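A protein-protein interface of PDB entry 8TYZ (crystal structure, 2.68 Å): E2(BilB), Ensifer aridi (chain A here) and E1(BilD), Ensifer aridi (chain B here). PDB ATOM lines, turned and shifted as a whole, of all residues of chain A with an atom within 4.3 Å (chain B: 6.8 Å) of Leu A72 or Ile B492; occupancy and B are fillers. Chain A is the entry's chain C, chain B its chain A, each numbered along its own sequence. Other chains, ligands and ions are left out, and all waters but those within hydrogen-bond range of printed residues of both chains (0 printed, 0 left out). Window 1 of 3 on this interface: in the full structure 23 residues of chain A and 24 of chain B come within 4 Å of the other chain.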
ATOM      1  N   VAL A   7     -19.975  18.705 -14.768  1.00  0.00           N
ATOM      2  CA  VAL A   7     -20.588  20.017 -14.598  1.00  0.00           C
ATOM      3  C   VAL A   7     -21.323  20.061 -13.268  1.00  0.00           C
ATOM      4  O   VAL A   7     -21.955  19.074 -12.870  1.00  0.00           O
ATOM      5  CB  VAL A   7     -21.568  20.299 -15.757  1.00  0.00           C
ATOM      6  CG1 VAL A   7     -22.376  21.562 -15.505  1.00  0.00           C
ATOM      7  CG2 VAL A   7     -20.854  20.376 -17.073  1.00  0.00           C
ATOM      8  N   ASN A  69     -23.888  16.380 -18.176  1.00  0.00           N
ATOM      9  CA  ASN A  69     -23.102  17.567 -18.471  1.00  0.00           C
ATOM     10  C   ASN A  69     -23.818  18.502 -19.426  1.00  0.00           C
ATOM     11  O   ASN A  69     -23.157  19.266 -20.148  1.00  0.00           O
ATOM     12  CB  ASN A  69     -21.735  17.196 -19.042  1.00  0.00           C
ATOM     13  CG  ASN A  69     -20.830  16.660 -18.012  1.00  0.00           C
ATOM     14  OD1 ASN A  69     -20.883  17.072 -16.861  1.00  0.00           O
ATOM     15  ND2 ASN A  69     -19.981  15.721 -18.407  1.00  0.00           N
ATOM     16  N   TYR A  70     -25.150  18.453 -19.464  1.00  0.00           N
ATOM     17  CA  TYR A  70     -25.866  19.099 -20.549  1.00  0.00           C
ATOM     18  C   TYR A  70     -25.748  20.588 -20.417  1.00  0.00           C
ATOM     19  O   TYR A  70     -26.210  21.194 -19.445  1.00  0.00           O
ATOM     20  CB  TYR A  70     -27.328  18.726 -20.608  1.00  0.00           C
ATOM     21  CG  TYR A  70     -28.137  19.527 -21.639  1.00  0.00           C
ATOM     22  CD1 TYR A  70     -29.167  20.358 -21.222  1.00  0.00           C
ATOM     23  CD2 TYR A  70     -27.911  19.409 -23.018  1.00  0.00           C
ATOM     24  CE1 TYR A  70     -29.948  21.050 -22.126  1.00  0.00           C
ATOM     25  CE2 TYR A  70     -28.691  20.113 -23.937  1.00  0.00           C
ATOM     26  CZ  TYR A  70     -29.712  20.930 -23.478  1.00  0.00           C
ATOM     27  OH  TYR A  70     -30.519  21.637 -24.347  1.00  0.00           O
ATOM     28  N   ASP A  71     -24.918  21.079 -21.311  1.00  0.00           N
ATOM     29  CA  ASP A  71     -25.244  22.018 -22.368  1.00  0.00           C
ATOM     30  C   ASP A  71     -23.880  22.583 -22.681  1.00  0.00           C
ATOM     31  O   ASP A  71     -23.620  23.028 -23.798  1.00  0.00           O
ATOM     32  CB  ASP A  71     -26.355  22.981 -21.965  1.00  0.00           C
ATOM     33  CG  ASP A  71     -25.992  24.380 -22.119  1.00  0.00           C
ATOM     34  OD1 ASP A  71     -25.109  24.803 -21.355  1.00  0.00           O
ATOM     35  OD2 ASP A  71     -26.616  25.047 -22.969  1.00  0.00           O
ATOM     36  N   LEU A  72     -22.967  22.430 -21.711  1.00  0.00           N
ATOM     37  CA  LEU A  72     -21.537  22.348 -22.022  1.00  0.00           C
ATOM     38  C   LEU A  72     -21.248  21.185 -22.961  1.00  0.00           C
ATOM     39  O   LEU A  72     -20.412  21.300 -23.863  1.00  0.00           O
ATOM     40  CB  LEU A  72     -20.716  22.202 -20.736  1.00  0.00           C
ATOM     41  CG  LEU A  72     -19.204  22.130 -20.928  1.00  0.00           C
ATOM     42  CD1 LEU A  72     -18.776  23.288 -21.803  1.00  0.00           C
ATOM     43  CD2 LEU A  72     -18.453  22.168 -19.623  1.00  0.00           C
ATOM     44  N   ARG A  73     -21.922  20.035 -22.746  1.00  0.00           N
ATOM     45  CA  ARG A  73     -21.845  18.907 -23.655  1.00  0.00           C
ATOM     46  C   ARG A  73     -23.211  18.650 -24.279  1.00  0.00           C
ATOM     47  O   ARG A  73     -24.232  18.878 -23.620  1.00  0.00           O
ATOM     48  CB  ARG A  73     -21.369  17.644 -22.927  1.00  0.00           C
ATOM     49  CG  ARG A  73     -19.907  17.670 -22.532  1.00  0.00           C
ATOM     50  CD  ARG A  73     -19.050  17.248 -23.677  1.00  0.00           C
ATOM     51  NE  ARG A  73     -19.008  15.801 -23.838  1.00  0.00           N
ATOM     52  CZ  ARG A  73     -18.761  15.191 -24.988  1.00  0.00           C
ATOM     53  NH1 ARG A  73     -18.627  15.872 -26.111  1.00  0.00           N
ATOM     54  NH2 ARG A  73     -18.651  13.868 -25.017  1.00  0.00           N
ATOM     55  N   TRP A 156     -19.258  21.552 -30.892  1.00  0.00           N
ATOM     56  CA  TRP A 156     -20.569  21.868 -30.336  1.00  0.00           C
ATOM     57  C   TRP A 156     -20.657  23.308 -29.854  1.00  0.00           C
ATOM     58  O   TRP A 156     -21.699  23.957 -30.018  1.00  0.00           O
ATOM     59  CB  TRP A 156     -20.882  20.883 -29.207  1.00  0.00           C
ATOM     60  CG  TRP A 156     -21.873  21.357 -28.207  1.00  0.00           C
ATOM     61  CD1 TRP A 156     -21.625  21.693 -26.911  1.00  0.00           C
ATOM     62  CD2 TRP A 156     -23.272  21.554 -28.412  1.00  0.00           C
ATOM     63  NE1 TRP A 156     -22.781  22.092 -26.294  1.00  0.00           N
ATOM     64  CE2 TRP A 156     -23.810  22.007 -27.193  1.00  0.00           C
ATOM     65  CE3 TRP A 156     -24.125  21.395 -29.509  1.00  0.00           C
ATOM     66  CZ2 TRP A 156     -25.160  22.303 -27.043  1.00  0.00           C
ATOM     67  CZ3 TRP A 156     -25.471  21.685 -29.353  1.00  0.00           C
ATOM     68  CH2 TRP A 156     -25.970  22.134 -28.134  1.00  0.00           C
ATOM     69  N   ARG A 160     -23.924  25.942 -29.420  1.00  0.00           N
ATOM     70  CA  ARG A 160     -24.503  26.102 -28.096  1.00  0.00           C
ATOM     71  C   ARG A 160     -25.345  27.373 -28.013  1.00  0.00           C
ATOM     72  O   ARG A 160     -25.022  28.394 -28.624  1.00  0.00           O
ATOM     73  CB  ARG A 160     -23.383  26.134 -27.059  1.00  0.00           C
ATOM     74  CG  ARG A 160     -23.768  25.648 -25.704  1.00  0.00           C
ATOM     75  CD  ARG A 160     -22.694  25.967 -24.688  1.00  0.00           C
ATOM     76  NE  ARG A 160     -23.346  26.254 -23.421  1.00  0.00           N
ATOM     77  CZ  ARG A 160     -23.694  27.468 -23.020  1.00  0.00           C
ATOM     78  NH1 ARG A 160     -23.307  28.549 -23.682  1.00  0.00           N
ATOM     79  NH2 ARG A 160     -24.450  27.604 -21.928  1.00  0.00           N
ATOM     80  N   VAL B 307     -11.616  22.485 -20.354  1.00  0.00           N
ATOM     81  CA  VAL B 307     -12.945  23.093 -20.329  1.00  0.00           C
ATOM     82  C   VAL B 307     -13.849  22.379 -19.326  1.00  0.00           C
ATOM     83  O   VAL B 307     -14.645  23.017 -18.624  1.00  0.00           O
ATOM     84  CB  VAL B 307     -13.540  23.085 -21.750  1.00  0.00           C
ATOM     85  CG1 VAL B 307     -14.990  23.547 -21.734  1.00  0.00           C
ATOM     86  CG2 VAL B 307     -12.699  23.929 -22.665  1.00  0.00           C
ATOM     87  N   ALA B 308     -13.726  21.051 -19.235  1.00  0.00           N
ATOM     88  CA  ALA B 308     -14.508  20.256 -18.292  1.00  0.00           C
ATOM     89  C   ALA B 308     -14.256  20.658 -16.851  1.00  0.00           C
ATOM     90  O   ALA B 308     -15.170  20.553 -16.021  1.00  0.00           O
ATOM     91  CB  ALA B 308     -14.196  18.780 -18.474  1.00  0.00           C
ATOM     92  N   VAL B 309     -13.033  21.085 -16.518  1.00  0.00           N
ATOM     93  CA  VAL B 309     -12.772  21.546 -15.155  1.00  0.00           C
ATOM     94  C   VAL B 309     -13.600  22.785 -14.857  1.00  0.00           C
ATOM     95  O   VAL B 309     -14.235  22.880 -13.800  1.00  0.00           O
ATOM     96  CB  VAL B 309     -11.271  21.804 -14.927  1.00  0.00           C
ATOM     97  CG1 VAL B 309     -11.058  22.478 -13.588  1.00  0.00           C
ATOM     98  CG2 VAL B 309     -10.516  20.520 -14.969  1.00  0.00           C
ATOM     99  N   GLN B 310     -13.617  23.744 -15.794  1.00  0.00           N
ATOM    100  CA  GLN B 310     -14.404  24.964 -15.630  1.00  0.00           C
ATOM    101  C   GLN B 310     -15.888  24.657 -15.443  1.00  0.00           C
ATOM    102  O   GLN B 310     -16.586  25.354 -14.696  1.00  0.00           O
ATOM    103  CB  GLN B 310     -14.207  25.876 -16.840  1.00  0.00           C
ATOM    104  CG  GLN B 310     -14.932  27.190 -16.715  1.00  0.00           C
ATOM    105  CD  GLN B 310     -14.352  28.044 -15.610  1.00  0.00           C
ATOM    106  OE1 GLN B 310     -14.701  27.906 -14.432  1.00  0.00           O
ATOM    107  NE2 GLN B 310     -13.446  28.924 -15.980  1.00  0.00           N
ATOM    108  N   GLY B 311     -16.384  23.623 -16.117  1.00  0.00           N
ATOM    109  CA  GLY B 311     -17.778  23.246 -15.970  1.00  0.00           C
ATOM    110  C   GLY B 311     -18.177  22.882 -14.554  1.00  0.00           C
ATOM    111  O   GLY B 311     -19.330  23.069 -14.171  1.00  0.00           O
ATOM    112  N   ALA B 312     -17.244  22.347 -13.760  1.00  0.00           N
ATOM    113  CA  ALA B 312     -17.551  22.024 -12.366  1.00  0.00           C
ATOM    114  C   ALA B 312     -17.671  23.265 -11.496  1.00  0.00           C
ATOM    115  O   ALA B 312     -18.055  23.145 -10.330  1.00  0.00           O
ATOM    116  CB  ALA B 312     -16.497  21.089 -11.776  1.00  0.00           C
ATOM    117  N   LEU B 313     -17.347  24.436 -12.044  1.00  0.00           N
ATOM    118  CA  LEU B 313     -17.459  25.750 -11.431  1.00  0.00           C
ATOM    119  C   LEU B 313     -16.626  25.885 -10.159  1.00  0.00           C
ATOM    120  O   LEU B 313     -17.183  26.081  -9.072  1.00  0.00           O
ATOM    121  CB  LEU B 313     -18.927  26.065 -11.166  1.00  0.00           C
ATOM    122  CG  LEU B 313     -19.656  26.306 -12.483  1.00  0.00           C
ATOM    123  CD1 LEU B 313     -21.072  26.767 -12.258  1.00  0.00           C
ATOM    124  CD2 LEU B 313     -18.894  27.328 -13.296  1.00  0.00           C
ATOM    125  N   PHE B 334     -14.919  33.022 -12.327  1.00  0.00           N
ATOM    126  CA  PHE B 334     -15.991  32.870 -13.304  1.00  0.00           C
ATOM    127  C   PHE B 334     -16.902  34.089 -13.355  1.00  0.00           C
ATOM    128  O   PHE B 334     -17.320  34.511 -14.439  1.00  0.00           O
ATOM    129  CB  PHE B 334     -16.795  31.620 -12.964  1.00  0.00           C
ATOM    130  CG  PHE B 334     -17.751  31.200 -14.010  1.00  0.00           C
ATOM    131  CD1 PHE B 334     -17.306  30.605 -15.164  1.00  0.00           C
ATOM    132  CD2 PHE B 334     -19.106  31.347 -13.810  1.00  0.00           C
ATOM    133  CE1 PHE B 334     -18.196  30.182 -16.104  1.00  0.00           C
ATOM    134  CE2 PHE B 334     -20.005  30.934 -14.753  1.00  0.00           C
ATOM    135  CZ  PHE B 334     -19.560  30.351 -15.890  1.00  0.00           C
ATOM    136  N   CYS B 340     -13.065  33.380 -18.604  1.00  0.00           N
ATOM    137  CA  CYS B 340     -13.050  32.143 -17.853  1.00  0.00           C
ATOM    138  C   CYS B 340     -12.154  31.163 -18.595  1.00  0.00           C
ATOM    139  O   CYS B 340     -11.669  31.448 -19.694  1.00  0.00           O
ATOM    140  CB  CYS B 340     -14.465  31.590 -17.699  1.00  0.00           C
ATOM    141  SG  CYS B 340     -15.105  30.833 -19.177  1.00  0.00           S
ATOM    142  N   CYS B 342     -12.961  28.561 -20.103  1.00  0.00           N
ATOM    143  CA  CYS B 342     -13.569  28.110 -21.350  1.00  0.00           C
ATOM    144  C   CYS B 342     -13.345  29.115 -22.484  1.00  0.00           C
ATOM    145  O   CYS B 342     -13.246  28.711 -23.652  1.00  0.00           O
ATOM    146  CB  CYS B 342     -15.054  27.830 -21.122  1.00  0.00           C
ATOM    147  SG  CYS B 342     -15.900  26.935 -22.437  1.00  0.00           S
ATOM    148  N   CYS B 343     -13.237  30.416 -22.160  1.00  0.00           N
ATOM    149  CA  CYS B 343     -12.982  31.444 -23.169  1.00  0.00           C
ATOM    150  C   CYS B 343     -11.694  31.155 -23.913  1.00  0.00           C
ATOM    151  O   CYS B 343     -11.611  31.327 -25.136  1.00  0.00           O
ATOM    152  CB  CYS B 343     -12.884  32.827 -22.519  1.00  0.00           C
ATOM    153  SG  CYS B 343     -14.386  33.455 -21.778  1.00  0.00           S
ATOM    154  N   MET B 346     -12.422  28.446 -26.612  1.00  0.00           N
ATOM    155  CA  MET B 346     -13.600  28.545 -27.468  1.00  0.00           C
ATOM    156  C   MET B 346     -13.224  28.319 -28.933  1.00  0.00           C
ATOM    157  O   MET B 346     -12.136  28.716 -29.367  1.00  0.00           O
ATOM    158  CB  MET B 346     -14.262  29.912 -27.318  1.00  0.00           C
ATOM    159  CG  MET B 346     -15.155  30.000 -26.109  1.00  0.00           C
ATOM    160  SD  MET B 346     -16.567  28.875 -26.129  1.00  0.00           S
ATOM    161  CE  MET B 346     -17.713  29.724 -27.204  1.00  0.00           C
ATOM    162  N   GLY B 489     -21.578  34.940 -26.824  1.00  0.00           N
ATOM    163  CA  GLY B 489     -22.709  34.473 -26.062  1.00  0.00           C
ATOM    164  C   GLY B 489     -22.776  32.970 -25.904  1.00  0.00           C
ATOM    165  O   GLY B 489     -23.611  32.482 -25.135  1.00  0.00           O
ATOM    166  N   ARG B 490     -21.914  32.225 -26.585  1.00  0.00           N
ATOM    167  CA  ARG B 490     -21.933  30.777 -26.553  1.00  0.00           C
ATOM    168  C   ARG B 490     -21.039  30.176 -25.469  1.00  0.00           C
ATOM    169  O   ARG B 490     -21.091  28.962 -25.252  1.00  0.00           O
ATOM    170  CB  ARG B 490     -21.541  30.244 -27.928  1.00  0.00           C
ATOM    171  CG  ARG B 490     -22.415  30.811 -29.024  1.00  0.00           C
ATOM    172  CD  ARG B 490     -22.065  30.270 -30.402  1.00  0.00           C
ATOM    173  NE  ARG B 490     -20.624  30.104 -30.596  1.00  0.00           N
ATOM    174  CZ  ARG B 490     -19.840  30.913 -31.300  1.00  0.00           C
ATOM    175  NH1 ARG B 490     -20.321  31.988 -31.905  1.00  0.00           N
ATOM    176  NH2 ARG B 490     -18.541  30.633 -31.402  1.00  0.00           N
ATOM    177  N   CYS B 491     -20.249  30.984 -24.772  1.00  0.00           N
ATOM    178  CA  CYS B 491     -19.426  30.482 -23.687  1.00  0.00           C
ATOM    179  C   CYS B 491     -20.267  30.332 -22.423  1.00  0.00           C
ATOM    180  O   CYS B 491     -21.280  31.012 -22.247  1.00  0.00           O
ATOM    181  CB  CYS B 491     -18.240  31.426 -23.437  1.00  0.00           C
ATOM    182  SG  CYS B 491     -16.898  30.788 -22.369  1.00  0.00           S
ATOM    183  N   ILE B 492     -19.825  29.437 -21.531  1.00  0.00           N
ATOM    184  CA  ILE B 492     -20.581  29.157 -20.323  1.00  0.00           C
ATOM    185  C   ILE B 492     -20.512  30.305 -19.320  1.00  0.00           C
ATOM    186  O   ILE B 492     -21.327  30.335 -18.389  1.00  0.00           O
ATOM    187  CB  ILE B 492     -20.137  27.826 -19.672  1.00  0.00           C
ATOM    188  CG1 ILE B 492     -18.664  27.843 -19.266  1.00  0.00           C
ATOM    189  CG2 ILE B 492     -20.386  26.632 -20.591  1.00  0.00           C
ATOM    190  CD1 ILE B 492     -18.236  26.591 -18.542  1.00  0.00           C
ATOM    191  N   CYS B 493     -19.597  31.275 -19.479  1.00  0.00           N
ATOM    192  CA  CYS B 493     -19.614  32.423 -18.569  1.00  0.00           C
ATOM    193  C   CYS B 493     -20.631  33.479 -18.969  1.00  0.00           C
ATOM    194  O   CYS B 493     -20.808  34.455 -18.231  1.00  0.00           O
ATOM    195  CB  CYS B 493     -18.230  33.070 -18.423  1.00  0.00           C
ATOM    196  SG  CYS B 493     -17.399  33.564 -19.937  1.00  0.00           S
ATOM    197  N   SER B 494     -21.315  33.275 -20.094  1.00  0.00           N
ATOM    198  CA  SER B 494     -22.466  34.064 -20.510  1.00  0.00           C
ATOM    199  C   SER B 494     -23.771  33.506 -19.972  1.00  0.00           C
ATOM    200  O   SER B 494     -24.782  34.221 -19.967  1.00  0.00           O
ATOM    201  CB  SER B 494     -22.564  34.119 -22.046  1.00  0.00           C
ATOM    202  OG  SER B 494     -21.354  34.550 -22.658  1.00  0.00           O
ATOM    203  N   ASP B 495     -23.763  32.257 -19.505  1.00  0.00           N
ATOM    204  CA  ASP B 495     -24.976  31.489 -19.238  1.00  0.00           C
ATOM    205  C   ASP B 495     -25.497  31.733 -17.824  1.00  0.00           C
ATOM    206  O   ASP B 495     -24.780  31.500 -16.845  1.00  0.00           O
ATOM    207  CB  ASP B 495     -24.695  30.004 -19.449  1.00  0.00           C
ATOM    208  CG  ASP B 495     -25.939  29.180 -19.433  1.00  0.00           C
ATOM    209  OD1 ASP B 495     -26.699  29.253 -18.445  1.00  0.00           O
ATOM    210  OD2 ASP B 495     -26.165  28.447 -20.419  1.00  0.00           O
ATOM    211  N   GLU B 496     -26.764  32.162 -17.724  1.00  0.00           N
ATOM    212  CA  GLU B 496     -27.312  32.591 -16.438  1.00  0.00           C
ATOM    213  C   GLU B 496     -27.403  31.444 -15.433  1.00  0.00           C
ATOM    214  O   GLU B 496     -27.288  31.674 -14.222  1.00  0.00           O
ATOM    215  CB  GLU B 496     -28.686  33.230 -16.642  1.00  0.00           C
ATOM    216  CG  GLU B 496     -28.666  34.554 -17.421  1.00  0.00           C
ATOM    217  CD  GLU B 496     -27.943  35.683 -16.683  1.00  0.00           C
ATOM    218  OE1 GLU B 496     -27.646  35.527 -15.472  1.00  0.00           O
ATOM    219  OE2 GLU B 496     -27.671  36.728 -17.324  1.00  0.00           O
ATOM    220  N   ASP B 497     -27.604  30.213 -15.913  1.00  0.00           N
ATOM    221  CA  ASP B 497     -27.623  29.050 -15.032  1.00  0.00           C
ATOM    222  C   ASP B 497     -26.247  28.796 -14.422  1.00  0.00           C
ATOM    223  O   ASP B 497     -26.126  28.569 -13.214  1.00  0.00           O
ATOM    224  CB  ASP B 497     -28.110  27.831 -15.815  1.00  0.00           C
ATOM    225  CG  ASP B 497     -29.572  27.943 -16.224  1.00  0.00           C
ATOM    226  OD1 ASP B 497     -30.411  28.336 -15.376  1.00  0.00           O
ATOM    227  OD2 ASP B 497     -29.884  27.634 -17.394  1.00  0.00           O
ATOM    228  N   PHE B 498     -25.192  28.836 -15.245  1.00  0.00           N
ATOM    229  CA  PHE B 498     -23.834  28.683 -14.725  1.00  0.00           C
ATOM    230  C   PHE B 498     -23.494  29.775 -13.715  1.00  0.00           C
ATOM    231  O   PHE B 498     -22.866  29.502 -12.685  1.00  0.00           O
ATOM    232  CB  PHE B 498     -22.829  28.688 -15.876  1.00  0.00           C
ATOM    233  CG  PHE B 498     -22.666  27.351 -16.559  1.00  0.00           C
ATOM    234  CD1 PHE B 498     -23.353  27.060 -17.730  1.00  0.00           C
ATOM    235  CD2 PHE B 498     -21.817  26.385 -16.031  1.00  0.00           C
ATOM    236  CE1 PHE B 498     -23.192  25.836 -18.361  1.00  0.00           C
ATOM    237  CE2 PHE B 498     -21.657  25.157 -16.656  1.00  0.00           C
ATOM    238  CZ  PHE B 498     -22.345  24.886 -17.823  1.00  0.00           C
ATOM    239  N   ILE B 499     -23.892  31.018 -13.998  1.00  0.00           N
ATOM    240  CA  ILE B 499     -23.612  32.134 -13.100  1.00  0.00           C
ATOM    241  C   ILE B 499     -24.388  31.998 -11.796  1.00  0.00           C
ATOM    242  O   ILE B 499     -23.906  32.412 -10.734  1.00  0.00           O
ATOM    243  CB  ILE B 499     -23.931  33.466 -13.811  1.00  0.00           C
ATOM    244  CG1 ILE B 499     -23.119  33.577 -15.101  1.00  0.00           C
ATOM    245  CG2 ILE B 499     -23.670  34.661 -12.904  1.00  0.00           C
ATOM    246  CD1 ILE B 499     -23.390  34.815 -15.890  1.00  0.00           C
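Among the printed residues, merely in contact across the chains: Val A7 with Gly B311 (3.3 Å), Val A7 with Phe B498 (3.8 Å), Asp A71 with Asp B495 (3.9 Å), Asp A71 with Phe B498 (3.7 Å), Leu A72 with Val B307 (3.8 Å), Leu A72 with Gly B311 (3.9 Å) and Leu A72 with Ile B492 (3.9 Å).
Of the 8 printed residues of chain A, 4 touch a printed residue of chain B. Hydrophobic or aromatic side chains of chain A that line the printed part of chain B: Val A7 and Leu A72. Along chain A the printed residues that touch a printed residue of chain B span positions 7 to 160. Of the 23 printed residues of chain B, 7 touch a printed residue of chain A. Hydrophobic or aromatic side chains of chain B that line the printed part of chain A: Val B307, Ile B492 and Phe B498. Among the printed residues, Asp or Glu carboxylates within 4 Å of a Lys or Arg side-chain nitrogen of the other chain: Arg A160 with Asp B495 (2.4 Å).
Printed residues of chain B within 4 Å of Val A7: Gly B311 and Phe B498. Of the printed residues of chain B, Arg A160 touches Arg B490, Cys B491 and Asp B495. Of the printed residues of chain A, Val B307 touches Leu A72. Of the printed residues of chain A, Cys B491 touches Arg A160 (3.5 Å). Ile B492 touches just one residue of chain A: Leu A72. The nearest residue of chain B that does not touch Leu A72 is Phe B498 (4.3 Å). The nearest residue of chain A that does not touch Ile B492 is Arg A160 (4.1 Å).
The backbone carbonyl oxygen (O) of Cys B491 lies within hydrogen-bond range of the guanidinium group (NH1) of Arg A160 (3.5 Å). The backbone carbonyl oxygen (O) of Arg B490 sits at hydrogen-bond distance from the guanidinium group (NH1) of Arg A160, at 2.7 Å. The guanidinium group (NH2) of Arg A160 lies within salt-bridge range of the side-chain carboxylate (OD2) of Asp B495, 2.4 Å away.
The side-chain carboxylate of Asp A71 is in salt-bridge range of the guanidinium group of Arg A160 (2.9 Å). The backbone carbonyl oxygen (O) of Asp A71 is in hydrogen-bond range of the indole nitrogen (NE1) of Trp A156, 2.8 Å away. The backbone NH of Val A7 sits at hydrogen-bond distance from the side-chain amide oxygen of Asn A69 (2.8 Å). OD1 of Asp B495 is in hydrogen-bond range of N of Asp B497 (2.9 Å). O of Leu A72 sits close to NE1 of Trp A156 (3.5 Å).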
